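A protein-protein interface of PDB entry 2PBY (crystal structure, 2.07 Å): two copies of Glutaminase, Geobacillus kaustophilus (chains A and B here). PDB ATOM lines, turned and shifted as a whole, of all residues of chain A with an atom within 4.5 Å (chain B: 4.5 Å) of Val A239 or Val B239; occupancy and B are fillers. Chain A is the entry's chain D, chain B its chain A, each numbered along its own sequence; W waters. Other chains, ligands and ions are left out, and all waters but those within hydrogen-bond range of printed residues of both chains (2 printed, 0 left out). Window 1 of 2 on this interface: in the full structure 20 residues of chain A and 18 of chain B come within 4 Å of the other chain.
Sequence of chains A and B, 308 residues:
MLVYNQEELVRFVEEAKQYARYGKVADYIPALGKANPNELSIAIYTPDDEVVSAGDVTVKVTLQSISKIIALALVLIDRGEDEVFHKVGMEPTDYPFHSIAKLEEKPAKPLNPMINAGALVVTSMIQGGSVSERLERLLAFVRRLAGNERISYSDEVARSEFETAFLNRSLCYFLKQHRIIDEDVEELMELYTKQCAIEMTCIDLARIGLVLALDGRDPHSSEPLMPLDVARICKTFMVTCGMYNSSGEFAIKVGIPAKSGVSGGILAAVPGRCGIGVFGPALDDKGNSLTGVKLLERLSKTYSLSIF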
ATOM      1  N   LYS A 235     -18.989 -35.694  24.247  1.00  0.00           N
ATOM      2  CA  LYS A 235     -17.666 -35.143  24.539  1.00  0.00           C
ATOM      3  C   LYS A 235     -17.325 -33.990  23.597  1.00  0.00           C
ATOM      4  O   LYS A 235     -16.620 -33.043  24.012  1.00  0.00           O
ATOM      5  CB  LYS A 235     -16.578 -36.200  24.540  1.00  0.00           C
ATOM      6  CG  LYS A 235     -16.520 -37.062  25.822  1.00  0.00           C
ATOM      7  CD  LYS A 235     -15.516 -38.266  25.725  1.00  0.00           C
ATOM      8  CE  LYS A 235     -15.971 -39.332  24.685  1.00  0.00           C
ATOM      9  NZ  LYS A 235     -15.000 -40.464  24.592  1.00  0.00           N
ATOM     10  N   THR A 236     -17.839 -34.016  22.358  1.00  0.00           N
ATOM     11  CA  THR A 236     -17.543 -32.913  21.454  1.00  0.00           C
ATOM     12  C   THR A 236     -18.208 -31.608  21.907  1.00  0.00           C
ATOM     13  O   THR A 236     -17.525 -30.542  21.907  1.00  0.00           O
ATOM     14  CB  THR A 236     -17.848 -33.191  19.919  1.00  0.00           C
ATOM     15  OG1 THR A 236     -19.254 -33.155  19.714  1.00  0.00           O
ATOM     16  CG2 THR A 236     -17.235 -34.542  19.397  1.00  0.00           C
ATOM     17  N   PHE A 237     -19.497 -31.670  22.297  1.00  0.00           N
ATOM     18  CA  PHE A 237     -20.178 -30.495  22.846  1.00  0.00           C
ATOM     19  C   PHE A 237     -19.521 -30.035  24.122  1.00  0.00           C
ATOM     20  O   PHE A 237     -19.544 -28.858  24.406  1.00  0.00           O
ATOM     21  CB  PHE A 237     -21.681 -30.748  23.117  1.00  0.00           C
ATOM     22  CG  PHE A 237     -22.524 -30.684  21.866  1.00  0.00           C
ATOM     23  CD1 PHE A 237     -22.765 -29.439  21.220  1.00  0.00           C
ATOM     24  CD2 PHE A 237     -23.001 -31.848  21.282  1.00  0.00           C
ATOM     25  CE1 PHE A 237     -23.505 -29.382  20.043  1.00  0.00           C
ATOM     26  CE2 PHE A 237     -23.750 -31.791  20.064  1.00  0.00           C
ATOM     27  CZ  PHE A 237     -23.987 -30.587  19.469  1.00  0.00           C
ATOM     28  N   MET A 238     -18.968 -30.970  24.901  1.00  0.00           N
ATOM     29  CA  MET A 238     -18.258 -30.639  26.126  1.00  0.00           C
ATOM     30  C   MET A 238     -16.935 -29.858  25.873  1.00  0.00           C
ATOM     31  O   MET A 238     -16.421 -29.187  26.752  1.00  0.00           O
ATOM     32  CB  MET A 238     -18.012 -31.899  26.976  1.00  0.00           C
ATOM     33  CG  MET A 238     -19.311 -32.467  27.567  1.00  0.00           C
ATOM     34  SD  MET A 238     -19.060 -34.120  28.191  1.00  0.00           S
ATOM     35  CE  MET A 238     -18.262 -33.757  29.777  1.00  0.00           C
ATOM     36  N   VAL A 239     -16.356 -29.990  24.691  1.00  0.00           N
ATOM     37  CA  VAL A 239     -15.181 -29.213  24.364  1.00  0.00           C
ATOM     38  C   VAL A 239     -15.576 -27.879  23.698  1.00  0.00           C
ATOM     39  O   VAL A 239     -15.011 -26.827  24.022  1.00  0.00           O
ATOM     40  CB  VAL A 239     -14.257 -30.046  23.461  1.00  0.00           C
ATOM     41  CG1 VAL A 239     -13.119 -29.188  22.891  1.00  0.00           C
ATOM     42  CG2 VAL A 239     -13.711 -31.197  24.267  1.00  0.00           C
ATOM     43  N   THR A 240     -16.568 -27.908  22.794  1.00  0.00           N
ATOM     44  CA  THR A 240     -16.890 -26.712  22.039  1.00  0.00           C
ATOM     45  C   THR A 240     -17.725 -25.688  22.788  1.00  0.00           C
ATOM     46  O   THR A 240     -17.629 -24.499  22.504  1.00  0.00           O
ATOM     47  CB  THR A 240     -17.535 -27.035  20.710  1.00  0.00           C
ATOM     48  OG1 THR A 240     -18.773 -27.740  20.948  1.00  0.00           O
ATOM     49  CG2 THR A 240     -16.507 -27.903  19.831  1.00  0.00           C
ATOM     50  N   CYS A 241     -18.568 -26.141  23.711  1.00  0.00           N
ATOM     51  CA  CYS A 241     -19.480 -25.218  24.394  1.00  0.00           C
ATOM     52  C   CYS A 241     -20.003 -25.768  25.694  1.00  0.00           C
ATOM     53  O   CYS A 241     -21.166 -25.563  25.997  1.00  0.00           O
ATOM     54  CB  CYS A 241     -20.669 -24.850  23.505  1.00  0.00           C
ATOM     55  SG  CYS A 241     -21.443 -26.246  22.630  1.00  0.00           S
ATOM     56  N   SER A 247     -15.873 -21.548  27.063  1.00  0.00           N
ATOM     57  CA  SER A 247     -15.354 -22.854  26.682  1.00  0.00           C
ATOM     58  C   SER A 247     -13.957 -22.761  26.027  1.00  0.00           C
ATOM     59  O   SER A 247     -13.128 -23.621  26.240  1.00  0.00           O
ATOM     60  CB  SER A 247     -16.317 -23.583  25.733  1.00  0.00           C
ATOM     61  OG  SER A 247     -17.546 -23.838  26.392  1.00  0.00           O
ATOM     62  N   PRO A 257     -12.648 -32.350  27.916  1.00  0.00           N
ATOM     63  CA  PRO A 257     -14.089 -32.264  27.766  1.00  0.00           C
ATOM     64  C   PRO A 257     -14.730 -32.017  29.128  1.00  0.00           C
ATOM     65  O   PRO A 257     -14.580 -32.863  30.014  1.00  0.00           O
ATOM     66  CB  PRO A 257     -14.491 -33.666  27.244  1.00  0.00           C
ATOM     67  CG  PRO A 257     -13.181 -34.213  26.451  1.00  0.00           C
ATOM     68  CD  PRO A 257     -12.070 -33.608  27.349  1.00  0.00           C
ATOM     69  N   ILE A 307      -6.035 -32.730  26.182  1.00  0.00           N
ATOM     70  CA  ILE A 307      -6.185 -33.544  24.974  1.00  0.00           C
ATOM     71  C   ILE A 307      -5.640 -32.841  23.716  1.00  0.00           C
ATOM     72  O   ILE A 307      -5.642 -33.427  22.591  1.00  0.00           O
ATOM     73  CB  ILE A 307      -7.693 -33.888  24.723  1.00  0.00           C
ATOM     74  CG1 ILE A 307      -8.485 -32.652  24.315  1.00  0.00           C
ATOM     75  CG2 ILE A 307      -8.355 -34.543  25.973  1.00  0.00           C
ATOM     76  CD1 ILE A 307      -9.954 -32.956  23.802  1.00  0.00           C
ATOM     77  N   PHE A 308      -5.181 -31.594  23.886  1.00  0.00           N
ATOM     78  CA  PHE A 308      -4.688 -30.771  22.753  1.00  0.00           C
ATOM     79  C   PHE A 308      -3.164 -30.894  22.510  1.00  0.00           C
ATOM     80  O   PHE A 308      -2.403 -31.454  23.352  1.00  0.00           O
ATOM     81  CB  PHE A 308      -5.082 -29.264  22.954  1.00  0.00           C
ATOM     82  CG  PHE A 308      -6.567 -29.032  22.951  1.00  0.00           C
ATOM     83  CD1 PHE A 308      -7.277 -28.953  21.737  1.00  0.00           C
ATOM     84  CD2 PHE A 308      -7.274 -28.952  24.141  1.00  0.00           C
ATOM     85  CE1 PHE A 308      -8.682 -28.782  21.745  1.00  0.00           C
ATOM     86  CE2 PHE A 308      -8.672 -28.775  24.135  1.00  0.00           C
ATOM     87  CZ  PHE A 308      -9.354 -28.696  22.943  1.00  0.00           C
ATOM     88  N   LYS B 235      -4.106 -25.176  18.480  1.00  0.00           N
ATOM     89  CA  LYS B 235      -4.924 -26.399  18.411  1.00  0.00           C
ATOM     90  C   LYS B 235      -6.304 -26.283  19.024  1.00  0.00           C
ATOM     91  O   LYS B 235      -7.263 -26.866  18.503  1.00  0.00           O
ATOM     92  CB  LYS B 235      -4.185 -27.606  18.945  1.00  0.00           C
ATOM     93  CG  LYS B 235      -3.095 -28.099  17.984  1.00  0.00           C
ATOM     94  CD  LYS B 235      -2.343 -29.274  18.598  1.00  0.00           C
ATOM     95  CE  LYS B 235      -1.420 -28.777  19.706  1.00  0.00           C
ATOM     96  NZ  LYS B 235      -0.667 -29.878  20.357  1.00  0.00           N
ATOM     97  N   THR B 236      -6.423 -25.542  20.121  1.00  0.00           N
ATOM     98  CA  THR B 236      -7.747 -25.321  20.681  1.00  0.00           C
ATOM     99  C   THR B 236      -8.674 -24.611  19.641  1.00  0.00           C
ATOM    100  O   THR B 236      -9.849 -25.042  19.412  1.00  0.00           O
ATOM    101  CB  THR B 236      -7.744 -24.533  22.016  1.00  0.00           C
ATOM    102  OG1 THR B 236      -7.381 -23.200  21.785  1.00  0.00           O
ATOM    103  CG2 THR B 236      -6.852 -25.123  23.134  1.00  0.00           C
ATOM    104  N   PHE B 237      -8.170 -23.560  18.991  1.00  0.00           N
ATOM    105  CA  PHE B 237      -8.972 -22.822  17.969  1.00  0.00           C
ATOM    106  C   PHE B 237      -9.262 -23.712  16.761  1.00  0.00           C
ATOM    107  O   PHE B 237     -10.296 -23.582  16.152  1.00  0.00           O
ATOM    108  CB  PHE B 237      -8.258 -21.563  17.441  1.00  0.00           C
ATOM    109  CG  PHE B 237      -8.303 -20.393  18.384  1.00  0.00           C
ATOM    110  CD1 PHE B 237      -9.507 -19.691  18.613  1.00  0.00           C
ATOM    111  CD2 PHE B 237      -7.150 -19.987  19.066  1.00  0.00           C
ATOM    112  CE1 PHE B 237      -9.538 -18.609  19.523  1.00  0.00           C
ATOM    113  CE2 PHE B 237      -7.202 -18.899  20.016  1.00  0.00           C
ATOM    114  CZ  PHE B 237      -8.380 -18.245  20.234  1.00  0.00           C
ATOM    115  N   MET B 238      -8.313 -24.570  16.378  1.00  0.00           N
ATOM    116  CA  MET B 238      -8.556 -25.535  15.321  1.00  0.00           C
ATOM    117  C   MET B 238      -9.622 -26.608  15.705  1.00  0.00           C
ATOM    118  O   MET B 238     -10.223 -27.233  14.822  1.00  0.00           O
ATOM    119  CB  MET B 238      -7.238 -26.226  14.937  1.00  0.00           C
ATOM    120  CG  MET B 238      -6.184 -25.243  14.389  1.00  0.00           C
ATOM    121  SD  MET B 238      -4.670 -26.094  14.029  1.00  0.00           S
ATOM    122  CE  MET B 238      -3.509 -25.634  15.232  1.00  0.00           C
ATOM    123  N   VAL B 239      -9.875 -26.826  16.998  1.00  0.00           N
ATOM    124  CA  VAL B 239     -11.035 -27.659  17.349  1.00  0.00           C
ATOM    125  C   VAL B 239     -12.370 -26.884  17.446  1.00  0.00           C
ATOM    126  O   VAL B 239     -13.419 -27.346  16.881  1.00  0.00           O
ATOM    127  CB  VAL B 239     -10.785 -28.467  18.625  1.00  0.00           C
ATOM    128  CG1 VAL B 239     -12.122 -29.132  19.162  1.00  0.00           C
ATOM    129  CG2 VAL B 239      -9.670 -29.493  18.378  1.00  0.00           C
ATOM    130  N   THR B 240     -12.357 -25.738  18.168  1.00  0.00           N
ATOM    131  CA  THR B 240     -13.565 -24.970  18.428  1.00  0.00           C
ATOM    132  C   THR B 240     -14.057 -24.159  17.196  1.00  0.00           C
ATOM    133  O   THR B 240     -15.280 -23.953  17.035  1.00  0.00           O
ATOM    134  CB  THR B 240     -13.394 -23.971  19.613  1.00  0.00           C
ATOM    135  OG1 THR B 240     -12.430 -22.981  19.248  1.00  0.00           O
ATOM    136  CG2 THR B 240     -12.969 -24.683  20.949  1.00  0.00           C
ATOM    137  N   CYS B 241     -13.146 -23.665  16.342  1.00  0.00           N
ATOM    138  CA  CYS B 241     -13.624 -22.869  15.209  1.00  0.00           C
ATOM    139  C   CYS B 241     -12.759 -22.857  13.957  1.00  0.00           C
ATOM    140  O   CYS B 241     -12.653 -21.808  13.315  1.00  0.00           O
ATOM    141  CB  CYS B 241     -13.839 -21.398  15.635  1.00  0.00           C
ATOM    142  SG  CYS B 241     -12.616 -20.745  16.785  1.00  0.00           S
ATOM    143  N   SER B 247     -17.343 -26.318  12.419  1.00  0.00           N
ATOM    144  CA  SER B 247     -16.415 -26.997  13.301  1.00  0.00           C
ATOM    145  C   SER B 247     -17.066 -28.069  14.160  1.00  0.00           C
ATOM    146  O   SER B 247     -16.441 -29.074  14.439  1.00  0.00           O
ATOM    147  CB  SER B 247     -15.715 -25.999  14.253  1.00  0.00           C
ATOM    148  OG  SER B 247     -15.093 -25.002  13.470  1.00  0.00           O
ATOM    149  N   PRO B 257      -8.121 -31.696  15.462  1.00  0.00           N
ATOM    150  CA  PRO B 257      -7.908 -30.263  15.217  1.00  0.00           C
ATOM    151  C   PRO B 257      -7.535 -30.019  13.750  1.00  0.00           C
ATOM    152  O   PRO B 257      -6.573 -30.656  13.249  1.00  0.00           O
ATOM    153  CB  PRO B 257      -6.713 -29.925  16.105  1.00  0.00           C
ATOM    154  CG  PRO B 257      -6.547 -31.089  17.099  1.00  0.00           C
ATOM    155  CD  PRO B 257      -7.165 -32.278  16.431  1.00  0.00           C
ATOM    156  N   ILE B 307      -9.694 -37.273  18.712  1.00  0.00           N
ATOM    157  CA  ILE B 307      -9.173 -36.992  20.103  1.00  0.00           C
ATOM    158  C   ILE B 307     -10.247 -37.136  21.218  1.00  0.00           C
ATOM    159  O   ILE B 307      -9.946 -37.075  22.435  1.00  0.00           O
ATOM    160  CB  ILE B 307      -8.577 -35.591  20.223  1.00  0.00           C
ATOM    161  CG1 ILE B 307      -9.695 -34.556  20.069  1.00  0.00           C
ATOM    162  CG2 ILE B 307      -7.471 -35.421  19.186  1.00  0.00           C
ATOM    163  CD1 ILE B 307      -9.214 -33.057  20.206  1.00  0.00           C
ATOM    164  N   PHE B 308     -11.491 -37.286  20.783  1.00  0.00           N
ATOM    165  CA  PHE B 308     -12.637 -37.286  21.688  1.00  0.00           C
ATOM    166  C   PHE B 308     -12.883 -38.693  22.245  1.00  0.00           C
ATOM    167  O   PHE B 308     -13.554 -38.839  23.271  1.00  0.00           O
ATOM    168  CB  PHE B 308     -13.901 -36.726  20.979  1.00  0.00           C
ATOM    169  CG  PHE B 308     -13.739 -35.300  20.551  1.00  0.00           C
ATOM    170  CD1 PHE B 308     -13.907 -34.253  21.484  1.00  0.00           C
ATOM    171  CD2 PHE B 308     -13.355 -34.989  19.244  1.00  0.00           C
ATOM    172  CE1 PHE B 308     -13.722 -32.899  21.077  1.00  0.00           C
ATOM    173  CE2 PHE B 308     -13.164 -33.660  18.841  1.00  0.00           C
ATOM    174  CZ  PHE B 308     -13.321 -32.615  19.743  1.00  0.00           C
HETATM  175  O   HOH W   1     -12.544 -41.981  23.741  1.00  0.00           O
HETATM  176  O   HOH W   2       0.155 -32.024  22.747  1.00  0.00           O
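O of Thr B236 sits at hydrogen-bond distance from OG1 of Thr B240, 3.3 Å away.
The backbone carbonyl oxygen of Thr A236 sits at hydrogen-bond distance from the side-chain hydroxyl of Thr A240 (3.2 Å).
Lys A235 touches Phe B308, and with the chains exchanged Phe A308 touches Lys B235.
Thr A236 touches Phe B308, and with the chains exchanged Phe A308 touches Thr B236.
Val B239 touches its own counterpart, Val A239.
Val A239 touches Phe B308, and with the chains exchanged Phe A308 touches Val B239.
Of the 11 printed residues of chain A, 5 touch a printed residue of chain B.
Hydrophobic or aromatic side chains of chain A within 4 Å of the printed part of chain B: Val A239, Ile A307 and Phe A308.
Hydrophobic or aromatic side chains of chain B within 4 Å of the printed part of chain A: Val B239, Ile B307 and Phe B308.
Among the printed residues, no Asp or Glu carboxylate lies within 4 Å of a Lys or Arg side-chain nitrogen of the other chain.
Water W2 bridges O of Phe A308 (2.7 Å) and NZ of Lys B235 (3.3 Å).
Water W1 lies within hydrogen-bond range of NZ of Lys A235 (3.0 Å) and O of Phe B308 (3.3 Å).
Printed residues of chain B within 4 Å of Lys A235: Phe B308 (2.5 Å).
Of chain B, only Val B239 (3.9 Å) and Phe B308 (3.6 Å) come within 4 Å of Val A239.
Pro A257 touches none of the printed residues of chain B.
Printed residues of chain A within 4 Å of Thr B236: Phe A308 (3.7 Å).
Val B239 touches two residues of chain A.
Cys B241 touches none of the printed residues of chain A.
The nearest residue of chain A that does not touch Val B239 is Thr A240 (4.3 Å).
The nearest printed residue of chain A that does not touch Thr B236 is Val A239 (6.3 Å).
CG2 of Thr A236 touches CG of Phe B308, at 3.8 Å.
Val B239 touches Val A239 (CG1 to CG1, 3.9 Å).
CE1 of Phe B308 touches CG2 of Val A239, at 3.6 Å.
Ile B307 touches Ile A307.
C of Phe A308 touches NZ of Lys B235, 3.5 Å away.
Phe A308 touches Thr B236.
Phe A308 touches Val B239 (CE1 to CG2, 3.6 Å).
O of Phe B308 lies within hydrogen-bond range of NZ of Lys A235, 2.5 Å away.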
